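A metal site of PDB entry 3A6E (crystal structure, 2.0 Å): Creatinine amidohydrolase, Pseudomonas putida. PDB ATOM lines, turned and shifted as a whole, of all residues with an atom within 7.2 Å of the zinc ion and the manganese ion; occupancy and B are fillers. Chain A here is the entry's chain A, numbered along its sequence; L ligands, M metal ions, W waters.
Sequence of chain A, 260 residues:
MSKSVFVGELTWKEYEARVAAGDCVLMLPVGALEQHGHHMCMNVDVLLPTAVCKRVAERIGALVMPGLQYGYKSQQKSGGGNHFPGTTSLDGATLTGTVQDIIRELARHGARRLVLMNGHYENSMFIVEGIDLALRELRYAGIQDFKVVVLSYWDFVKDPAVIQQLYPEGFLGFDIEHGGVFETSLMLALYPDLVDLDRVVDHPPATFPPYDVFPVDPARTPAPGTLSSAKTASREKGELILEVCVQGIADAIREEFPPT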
ATOM      1  N   GLY A  31      11.699 -29.153  23.867  1.00  0.00           N
ATOM      2  CA  GLY A  31      11.705 -28.996  22.425  1.00  0.00           C
ATOM      3  C   GLY A  31      11.822 -30.270  21.610  1.00  0.00           C
ATOM      4  O   GLY A  31      11.152 -31.263  21.875  1.00  0.00           O
ATOM      5  N   ALA A  32      12.691 -30.232  20.600  1.00  0.00           N
ATOM      6  CA  ALA A  32      12.892 -31.387  19.725  1.00  0.00           C
ATOM      7  C   ALA A  32      14.004 -31.115  18.727  1.00  0.00           C
ATOM      8  O   ALA A  32      14.433 -29.971  18.561  1.00  0.00           O
ATOM      9  CB  ALA A  32      11.609 -31.687  18.965  1.00  0.00           C
ATOM     10  N   GLU A  34      14.309 -31.452  14.989  1.00  0.00           N
ATOM     11  CA  GLU A  34      13.418 -31.695  13.874  1.00  0.00           C
ATOM     12  C   GLU A  34      13.698 -30.824  12.663  1.00  0.00           C
ATOM     13  O   GLU A  34      14.072 -29.649  12.799  1.00  0.00           O
ATOM     14  CB  GLU A  34      11.984 -31.452  14.364  1.00  0.00           C
ATOM     15  CG  GLU A  34      10.859 -31.555  13.342  1.00  0.00           C
ATOM     16  CD  GLU A  34       9.541 -31.093  13.934  1.00  0.00           C
ATOM     17  OE1 GLU A  34       9.533 -30.007  14.526  1.00  0.00           O
ATOM     18  OE2 GLU A  34       8.517 -31.804  13.814  1.00  0.00           O
ATOM     19  N   GLN A  35      13.507 -31.393  11.477  1.00  0.00           N
ATOM     20  CA  GLN A  35      13.734 -30.664  10.244  1.00  0.00           C
ATOM     21  C   GLN A  35      12.854 -29.417  10.225  1.00  0.00           C
ATOM     22  O   GLN A  35      11.691 -29.455  10.647  1.00  0.00           O
ATOM     23  CB  GLN A  35      13.399 -31.552   9.037  1.00  0.00           C
ATOM     24  CG  GLN A  35      11.919 -31.937   8.884  1.00  0.00           C
ATOM     25  CD  GLN A  35      11.085 -30.854   8.211  1.00  0.00           C
ATOM     26  OE1 GLN A  35      11.604 -29.997   7.501  1.00  0.00           O
ATOM     27  NE2 GLN A  35       9.765 -30.914   8.421  1.00  0.00           N
ATOM     28  N   HIS A  36      13.419 -28.304   9.769  1.00  0.00           N
ATOM     29  CA  HIS A  36      12.685 -27.056   9.660  1.00  0.00           C
ATOM     30  C   HIS A  36      12.908 -26.417   8.303  1.00  0.00           C
ATOM     31  O   HIS A  36      13.254 -25.245   8.214  1.00  0.00           O
ATOM     32  CB  HIS A  36      13.095 -26.085  10.773  1.00  0.00           C
ATOM     33  CG  HIS A  36      12.329 -26.286  12.043  1.00  0.00           C
ATOM     34  ND1 HIS A  36      12.518 -27.390  12.855  1.00  0.00           N
ATOM     35  CD2 HIS A  36      11.332 -25.577  12.611  1.00  0.00           C
ATOM     36  CE1 HIS A  36      11.660 -27.349  13.864  1.00  0.00           C
ATOM     37  NE2 HIS A  36      10.927 -26.251  13.730  1.00  0.00           N
ATOM     38  N   MET A  40      16.197 -23.180   7.768  1.00  0.00           N
ATOM     39  CA  MET A  40      16.504 -23.079   9.191  1.00  0.00           C
ATOM     40  C   MET A  40      17.127 -24.359   9.738  1.00  0.00           C
ATOM     41  O   MET A  40      16.968 -25.423   9.156  1.00  0.00           O
ATOM     42  CB  MET A  40      15.256 -22.741  10.008  1.00  0.00           C
ATOM     43  CG  MET A  40      14.729 -21.340   9.819  1.00  0.00           C
ATOM     44  SD  MET A  40      13.577 -20.897  11.133  1.00  0.00           S
ATOM     45  CE  MET A  40      12.156 -21.896  10.691  1.00  0.00           C
ATOM     46  N   VAL A  44      15.518 -25.520  16.302  1.00  0.00           N
ATOM     47  CA  VAL A  44      14.579 -24.416  16.489  1.00  0.00           C
ATOM     48  C   VAL A  44      13.598 -24.617  17.654  1.00  0.00           C
ATOM     49  O   VAL A  44      13.361 -23.700  18.446  1.00  0.00           O
ATOM     50  CB  VAL A  44      13.747 -24.175  15.194  1.00  0.00           C
ATOM     51  CG1 VAL A  44      12.628 -23.171  15.462  1.00  0.00           C
ATOM     52  CG2 VAL A  44      14.669 -23.655  14.079  1.00  0.00           C
ATOM     53  N   ASP A  45      13.023 -25.822  17.766  1.00  0.00           N
ATOM     54  CA  ASP A  45      12.060 -26.116  18.825  1.00  0.00           C
ATOM     55  C   ASP A  45      12.664 -26.094  20.228  1.00  0.00           C
ATOM     56  O   ASP A  45      11.932 -26.120  21.209  1.00  0.00           O
ATOM     57  CB  ASP A  45      11.372 -27.453  18.577  1.00  0.00           C
ATOM     58  CG  ASP A  45      10.377 -27.389  17.438  1.00  0.00           C
ATOM     59  OD1 ASP A  45      10.187 -26.279  16.886  1.00  0.00           O
ATOM     60  OD2 ASP A  45       9.791 -28.420  17.083  1.00  0.00           O
ATOM     61  N   VAL A  46      13.983 -26.068  20.303  1.00  0.00           N
ATOM     62  CA  VAL A  46      14.665 -25.986  21.588  1.00  0.00           C
ATOM     63  C   VAL A  46      15.060 -24.527  21.787  1.00  0.00           C
ATOM     64  O   VAL A  46      14.818 -23.945  22.844  1.00  0.00           O
ATOM     65  CB  VAL A  46      15.965 -26.828  21.634  1.00  0.00           C
ATOM     66  CG1 VAL A  46      16.769 -26.463  22.891  1.00  0.00           C
ATOM     67  CG2 VAL A  46      15.635 -28.306  21.647  1.00  0.00           C
ATOM     68  N   LEU A  48      13.882 -21.675  20.524  1.00  0.00           N
ATOM     69  CA  LEU A  48      12.806 -20.717  20.754  1.00  0.00           C
ATOM     70  C   LEU A  48      12.176 -20.714  22.148  1.00  0.00           C
ATOM     71  O   LEU A  48      12.115 -19.663  22.781  1.00  0.00           O
ATOM     72  CB  LEU A  48      11.738 -20.885  19.662  1.00  0.00           C
ATOM     73  CG  LEU A  48      12.312 -20.549  18.279  1.00  0.00           C
ATOM     74  CD1 LEU A  48      11.202 -20.557  17.229  1.00  0.00           C
ATOM     75  CD2 LEU A  48      12.978 -19.166  18.319  1.00  0.00           C
ATOM     76  N   TYR A  72       8.729 -35.737  21.043  1.00  0.00           N
ATOM     77  CA  TYR A  72       7.953 -36.783  20.398  1.00  0.00           C
ATOM     78  C   TYR A  72       8.035 -36.738  18.873  1.00  0.00           C
ATOM     79  O   TYR A  72       8.356 -35.709  18.278  1.00  0.00           O
ATOM     80  CB  TYR A  72       6.489 -36.735  20.835  1.00  0.00           C
ATOM     81  CG  TYR A  72       5.680 -37.922  20.349  1.00  0.00           C
ATOM     82  CD1 TYR A  72       5.969 -39.217  20.794  1.00  0.00           C
ATOM     83  CD2 TYR A  72       4.693 -37.758  19.374  1.00  0.00           C
ATOM     84  CE1 TYR A  72       5.286 -40.319  20.282  1.00  0.00           C
ATOM     85  CE2 TYR A  72       4.013 -38.863  18.853  1.00  0.00           C
ATOM     86  CZ  TYR A  72       4.320 -40.132  19.306  1.00  0.00           C
ATOM     87  OH  TYR A  72       3.666 -41.219  18.765  1.00  0.00           O
ATOM     88  N   SER A  74       7.655 -36.374  15.084  1.00  0.00           N
ATOM     89  CA  SER A  74       7.089 -35.322  14.247  1.00  0.00           C
ATOM     90  C   SER A  74       5.897 -35.908  13.490  1.00  0.00           C
ATOM     91  O   SER A  74       5.990 -37.002  12.935  1.00  0.00           O
ATOM     92  CB  SER A  74       8.152 -34.837  13.250  1.00  0.00           C
ATOM     93  OG  SER A  74       7.634 -33.858  12.364  1.00  0.00           O
ATOM     94  N   SER A  78       1.616 -31.462  11.330  1.00  0.00           N
ATOM     95  CA  SER A  78       2.093 -30.443  12.260  1.00  0.00           C
ATOM     96  C   SER A  78       3.590 -30.162  12.114  1.00  0.00           C
ATOM     97  O   SER A  78       4.018 -29.014  12.209  1.00  0.00           O
ATOM     98  CB  SER A  78       1.775 -30.841  13.704  1.00  0.00           C
ATOM     99  OG  SER A  78       2.324 -32.106  14.040  1.00  0.00           O
ATOM    100  N   GLY A  79       4.375 -31.199  11.860  1.00  0.00           N
ATOM    101  CA  GLY A  79       5.809 -31.026  11.721  1.00  0.00           C
ATOM    102  C   GLY A  79       6.409 -31.590  10.443  1.00  0.00           C
ATOM    103  O   GLY A  79       7.630 -31.628  10.304  1.00  0.00           O
ATOM    104  N   GLY A 119       7.793 -26.248  22.940  1.00  0.00           N
ATOM    105  CA  GLY A 119       8.174 -25.561  21.722  1.00  0.00           C
ATOM    106  C   GLY A 119       7.990 -26.445  20.502  1.00  0.00           C
ATOM    107  O   GLY A 119       8.239 -26.014  19.377  1.00  0.00           O
ATOM    108  N   HIS A 120       7.567 -27.684  20.746  1.00  0.00           N
ATOM    109  CA  HIS A 120       7.338 -28.691  19.708  1.00  0.00           C
ATOM    110  C   HIS A 120       5.911 -29.190  19.916  1.00  0.00           C
ATOM    111  O   HIS A 120       5.640 -29.908  20.870  1.00  0.00           O
ATOM    112  CB  HIS A 120       8.342 -29.833  19.870  1.00  0.00           C
ATOM    113  CG  HIS A 120       8.149 -30.986  18.925  1.00  0.00           C
ATOM    114  ND1 HIS A 120       8.158 -30.841  17.554  1.00  0.00           N
ATOM    115  CD2 HIS A 120       8.039 -32.314  19.158  1.00  0.00           C
ATOM    116  CE1 HIS A 120       8.059 -32.026  16.987  1.00  0.00           C
ATOM    117  NE2 HIS A 120       7.994 -32.944  17.936  1.00  0.00           N
ATOM    118  N   TYR A 121       5.002 -28.798  19.007  1.00  0.00           N
ATOM    119  CA  TYR A 121       3.584 -29.142  19.088  1.00  0.00           C
ATOM    120  C   TYR A 121       3.249 -30.568  19.508  1.00  0.00           C
ATOM    121  O   TYR A 121       2.425 -30.778  20.404  1.00  0.00           O
ATOM    122  CB  TYR A 121       2.901 -28.868  17.737  1.00  0.00           C
ATOM    123  CG  TYR A 121       1.399 -29.014  17.781  1.00  0.00           C
ATOM    124  CD1 TYR A 121       0.608 -28.124  18.500  1.00  0.00           C
ATOM    125  CD2 TYR A 121       0.766 -30.059  17.100  1.00  0.00           C
ATOM    126  CE1 TYR A 121      -0.773 -28.253  18.540  1.00  0.00           C
ATOM    127  CE2 TYR A 121      -0.619 -30.202  17.144  1.00  0.00           C
ATOM    128  CZ  TYR A 121      -1.385 -29.297  17.864  1.00  0.00           C
ATOM    129  OH  TYR A 121      -2.755 -29.424  17.896  1.00  0.00           O
ATOM    130  N   GLU A 122       3.886 -31.543  18.873  1.00  0.00           N
ATOM    131  CA  GLU A 122       3.645 -32.950  19.149  1.00  0.00           C
ATOM    132  C   GLU A 122       3.931 -33.432  20.588  1.00  0.00           C
ATOM    133  O   GLU A 122       3.451 -34.484  20.993  1.00  0.00           O
ATOM    134  CB  GLU A 122       4.438 -33.827  18.154  1.00  0.00           C
ATOM    135  CG  GLU A 122       3.965 -33.691  16.691  1.00  0.00           C
ATOM    136  CD  GLU A 122       4.599 -32.533  15.922  1.00  0.00           C
ATOM    137  OE1 GLU A 122       4.902 -31.476  16.527  1.00  0.00           O
ATOM    138  OE2 GLU A 122       4.780 -32.669  14.697  1.00  0.00           O
ATOM    139  N   ASN A 123       4.717 -32.664  21.342  1.00  0.00           N
ATOM    140  CA  ASN A 123       5.069 -33.034  22.729  1.00  0.00           C
ATOM    141  C   ASN A 123       3.944 -32.942  23.742  1.00  0.00           C
ATOM    142  O   ASN A 123       3.928 -33.679  24.743  1.00  0.00           O
ATOM    143  CB  ASN A 123       6.175 -32.131  23.288  1.00  0.00           C
ATOM    144  CG  ASN A 123       7.520 -32.341  22.641  1.00  0.00           C
ATOM    145  OD1 ASN A 123       7.828 -33.411  22.140  1.00  0.00           O
ATOM    146  ND2 ASN A 123       8.343 -31.293  22.686  1.00  0.00           N
ATOM    147  N   TYR A 153       4.380 -21.579  23.953  1.00  0.00           N
ATOM    148  CA  TYR A 153       4.569 -20.144  23.816  1.00  0.00           C
ATOM    149  C   TYR A 153       3.776 -19.438  22.725  1.00  0.00           C
ATOM    150  O   TYR A 153       3.316 -18.313  22.933  1.00  0.00           O
ATOM    151  CB  TYR A 153       6.076 -19.806  23.697  1.00  0.00           C
ATOM    152  CG  TYR A 153       6.711 -20.151  22.366  1.00  0.00           C
ATOM    153  CD1 TYR A 153       6.631 -19.268  21.288  1.00  0.00           C
ATOM    154  CD2 TYR A 153       7.346 -21.373  22.164  1.00  0.00           C
ATOM    155  CE1 TYR A 153       7.174 -19.591  20.055  1.00  0.00           C
ATOM    156  CE2 TYR A 153       7.894 -21.704  20.935  1.00  0.00           C
ATOM    157  CZ  TYR A 153       7.807 -20.811  19.885  1.00  0.00           C
ATOM    158  OH  TYR A 153       8.292 -21.154  18.652  1.00  0.00           O
ATOM    159  N   TRP A 154       3.582 -20.085  21.586  1.00  0.00           N
ATOM    160  CA  TRP A 154       2.840 -19.463  20.494  1.00  0.00           C
ATOM    161  C   TRP A 154       1.367 -19.170  20.803  1.00  0.00           C
ATOM    162  O   TRP A 154       0.770 -18.271  20.195  1.00  0.00           O
ATOM    163  CB  TRP A 154       2.930 -20.327  19.226  1.00  0.00           C
ATOM    164  CG  TRP A 154       2.424 -21.728  19.392  1.00  0.00           C
ATOM    165  CD1 TRP A 154       1.125 -22.142  19.399  1.00  0.00           C
ATOM    166  CD2 TRP A 154       3.223 -22.904  19.594  1.00  0.00           C
ATOM    167  NE1 TRP A 154       1.062 -23.502  19.591  1.00  0.00           N
ATOM    168  CE2 TRP A 154       2.330 -23.995  19.718  1.00  0.00           C
ATOM    169  CE3 TRP A 154       4.595 -23.141  19.686  1.00  0.00           C
ATOM    170  CZ2 TRP A 154       2.776 -25.306  19.929  1.00  0.00           C
ATOM    171  CZ3 TRP A 154       5.041 -24.452  19.897  1.00  0.00           C
ATOM    172  CH2 TRP A 154       4.127 -25.508  20.014  1.00  0.00           C
ATOM    173  N   GLU A 177       1.905 -23.613  10.601  1.00  0.00           N
ATOM    174  CA  GLU A 177       3.103 -22.943  11.068  1.00  0.00           C
ATOM    175  C   GLU A 177       4.270 -23.813  11.535  1.00  0.00           C
ATOM    176  O   GLU A 177       4.631 -23.828  12.717  1.00  0.00           O
ATOM    177  CB  GLU A 177       2.753 -21.941  12.182  1.00  0.00           C
ATOM    178  CG  GLU A 177       2.053 -20.660  11.699  1.00  0.00           C
ATOM    179  CD  GLU A 177       2.904 -19.816  10.760  1.00  0.00           C
ATOM    180  OE1 GLU A 177       4.152 -19.921  10.805  1.00  0.00           O
ATOM    181  OE2 GLU A 177       2.320 -19.031   9.987  1.00  0.00           O
ATOM    182  N   HIS A 178       4.865 -24.548  10.598  1.00  0.00           N
ATOM    183  CA  HIS A 178       6.045 -25.342  10.901  1.00  0.00           C
ATOM    184  C   HIS A 178       7.082 -24.832   9.910  1.00  0.00           C
ATOM    185  O   HIS A 178       6.984 -25.112   8.718  1.00  0.00           O
ATOM    186  CB  HIS A 178       5.827 -26.837  10.678  1.00  0.00           C
ATOM    187  CG  HIS A 178       7.097 -27.640  10.811  1.00  0.00           C
ATOM    188  ND1 HIS A 178       7.824 -27.675  11.985  1.00  0.00           N
ATOM    189  CD2 HIS A 178       7.789 -28.364   9.910  1.00  0.00           C
ATOM    190  CE1 HIS A 178       8.922 -28.386  11.798  1.00  0.00           C
ATOM    191  NE2 HIS A 178       8.930 -28.812  10.544  1.00  0.00           N
ATOM    192  N   GLY A 179       8.057 -24.069  10.391  1.00  0.00           N
ATOM    193  CA  GLY A 179       9.070 -23.517   9.510  1.00  0.00           C
ATOM    194  C   GLY A 179       8.504 -22.371   8.685  1.00  0.00           C
ATOM    195  O   GLY A 179       9.094 -21.958   7.686  1.00  0.00           O
ATOM    196  N   GLU A 183       7.701 -19.024  13.218  1.00  0.00           N
ATOM    197  CA  GLU A 183       8.983 -19.460  13.767  1.00  0.00           C
ATOM    198  C   GLU A 183      10.172 -18.801  13.098  1.00  0.00           C
ATOM    199  O   GLU A 183      11.165 -18.510  13.744  1.00  0.00           O
ATOM    200  CB  GLU A 183       9.160 -20.957  13.614  1.00  0.00           C
ATOM    201  CG  GLU A 183       8.179 -21.812  14.356  1.00  0.00           C
ATOM    202  CD  GLU A 183       8.574 -23.254  14.291  1.00  0.00           C
ATOM    203  OE1 GLU A 183       8.991 -23.800  15.329  1.00  0.00           O
ATOM    204  OE2 GLU A 183       8.499 -23.830  13.184  1.00  0.00           O
HETATM  205 AS1  LIG L   1       6.270 -26.780  15.754  1.00  0.00          AS
HETATM  206  O1  LIG L   1       6.443 -28.009  16.987  1.00  0.00           O
HETATM  207  O2  LIG L   1       7.621 -26.965  14.674  1.00  0.00           O
HETATM  208  C1  LIG L   1       4.656 -27.076  14.679  1.00  0.00           C
HETATM  209  C2  LIG L   1       6.380 -24.990  16.536  1.00  0.00           C
HETATM  210 ZN    ZN M   1       9.336 -25.801  15.034  1.00  0.00          ZN
HETATM  211 MN    MN M   2       8.115 -29.193  16.031  1.00  0.00          MN
HETATM  212  O   HOH W   1       6.531 -30.024  14.861  1.00  0.00           O
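The zinc ion is bound by the side-chain carboxylate (OE1) of Glu 183 (2.1 Å), the side-chain carboxylate (OD1) of Asp 45 (2.1 Å), an oxygen (O2) of the ligand (2.1 Å) and a ring nitrogen (NE2) of His 36 (2.1 Å). Slightly farther from the zinc ion lies OE2 of Glu 183 (2.8 Å).
The backbone NH (N) of Gly 179 is in hydrogen-bond range of the side-chain carboxylate (OE2) of Glu 183 (2.8 Å). The backbone carbonyl oxygen (O) of Glu 34 is in hydrogen-bond range of a ring nitrogen (ND1) of His 36 (2.7 Å). OG of Ser 74 sits at hydrogen-bond distance from OE2 of Glu 34 (2.7 Å). ND1 of His 120 sits close to OE1 of Glu 122, at 3.5 Å. A ring nitrogen (NE2) of His 178 is in hydrogen-bond range of the backbone carbonyl oxygen (O) of Gly 79, at 3.1 Å. NE2 of His 178 sits at hydrogen-bond distance from O of Gln 35 (2.8 Å). OE2 of Glu 122 lies within hydrogen-bond range of N of Gly 79. The side-chain carboxylate of Glu 122 lies within hydrogen-bond range of the side-chain hydroxyl of Ser 78, 2.6 Å away.
Merely in contact with the zinc ion: His 178 (3.9 Å). Four residues have an atom within 4 Å of the zinc ion: His 36, Asp 45, His 178 and Glu 183.
The manganese ion is bound by the side-chain carboxylate (OD2) of Asp 45 (2.1 Å), water W1 (2.1 Å), the side-chain carboxylate (OE1) of Glu 34 (2.2 Å), a ring nitrogen (ND1) of His 120 (2.2 Å), an oxygen (O1) of the ligand (2.3 Å) and an oxygen (O2) of the ligand (2.7 Å).
Water W1 lies within hydrogen-bond range of OE1 of Glu 122 and OE2 of Glu 34.
Merely in contact with the manganese ion: Glu 122. The nearest printed residue that does not touch the manganese ion is Tyr 121 (4.3 Å).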
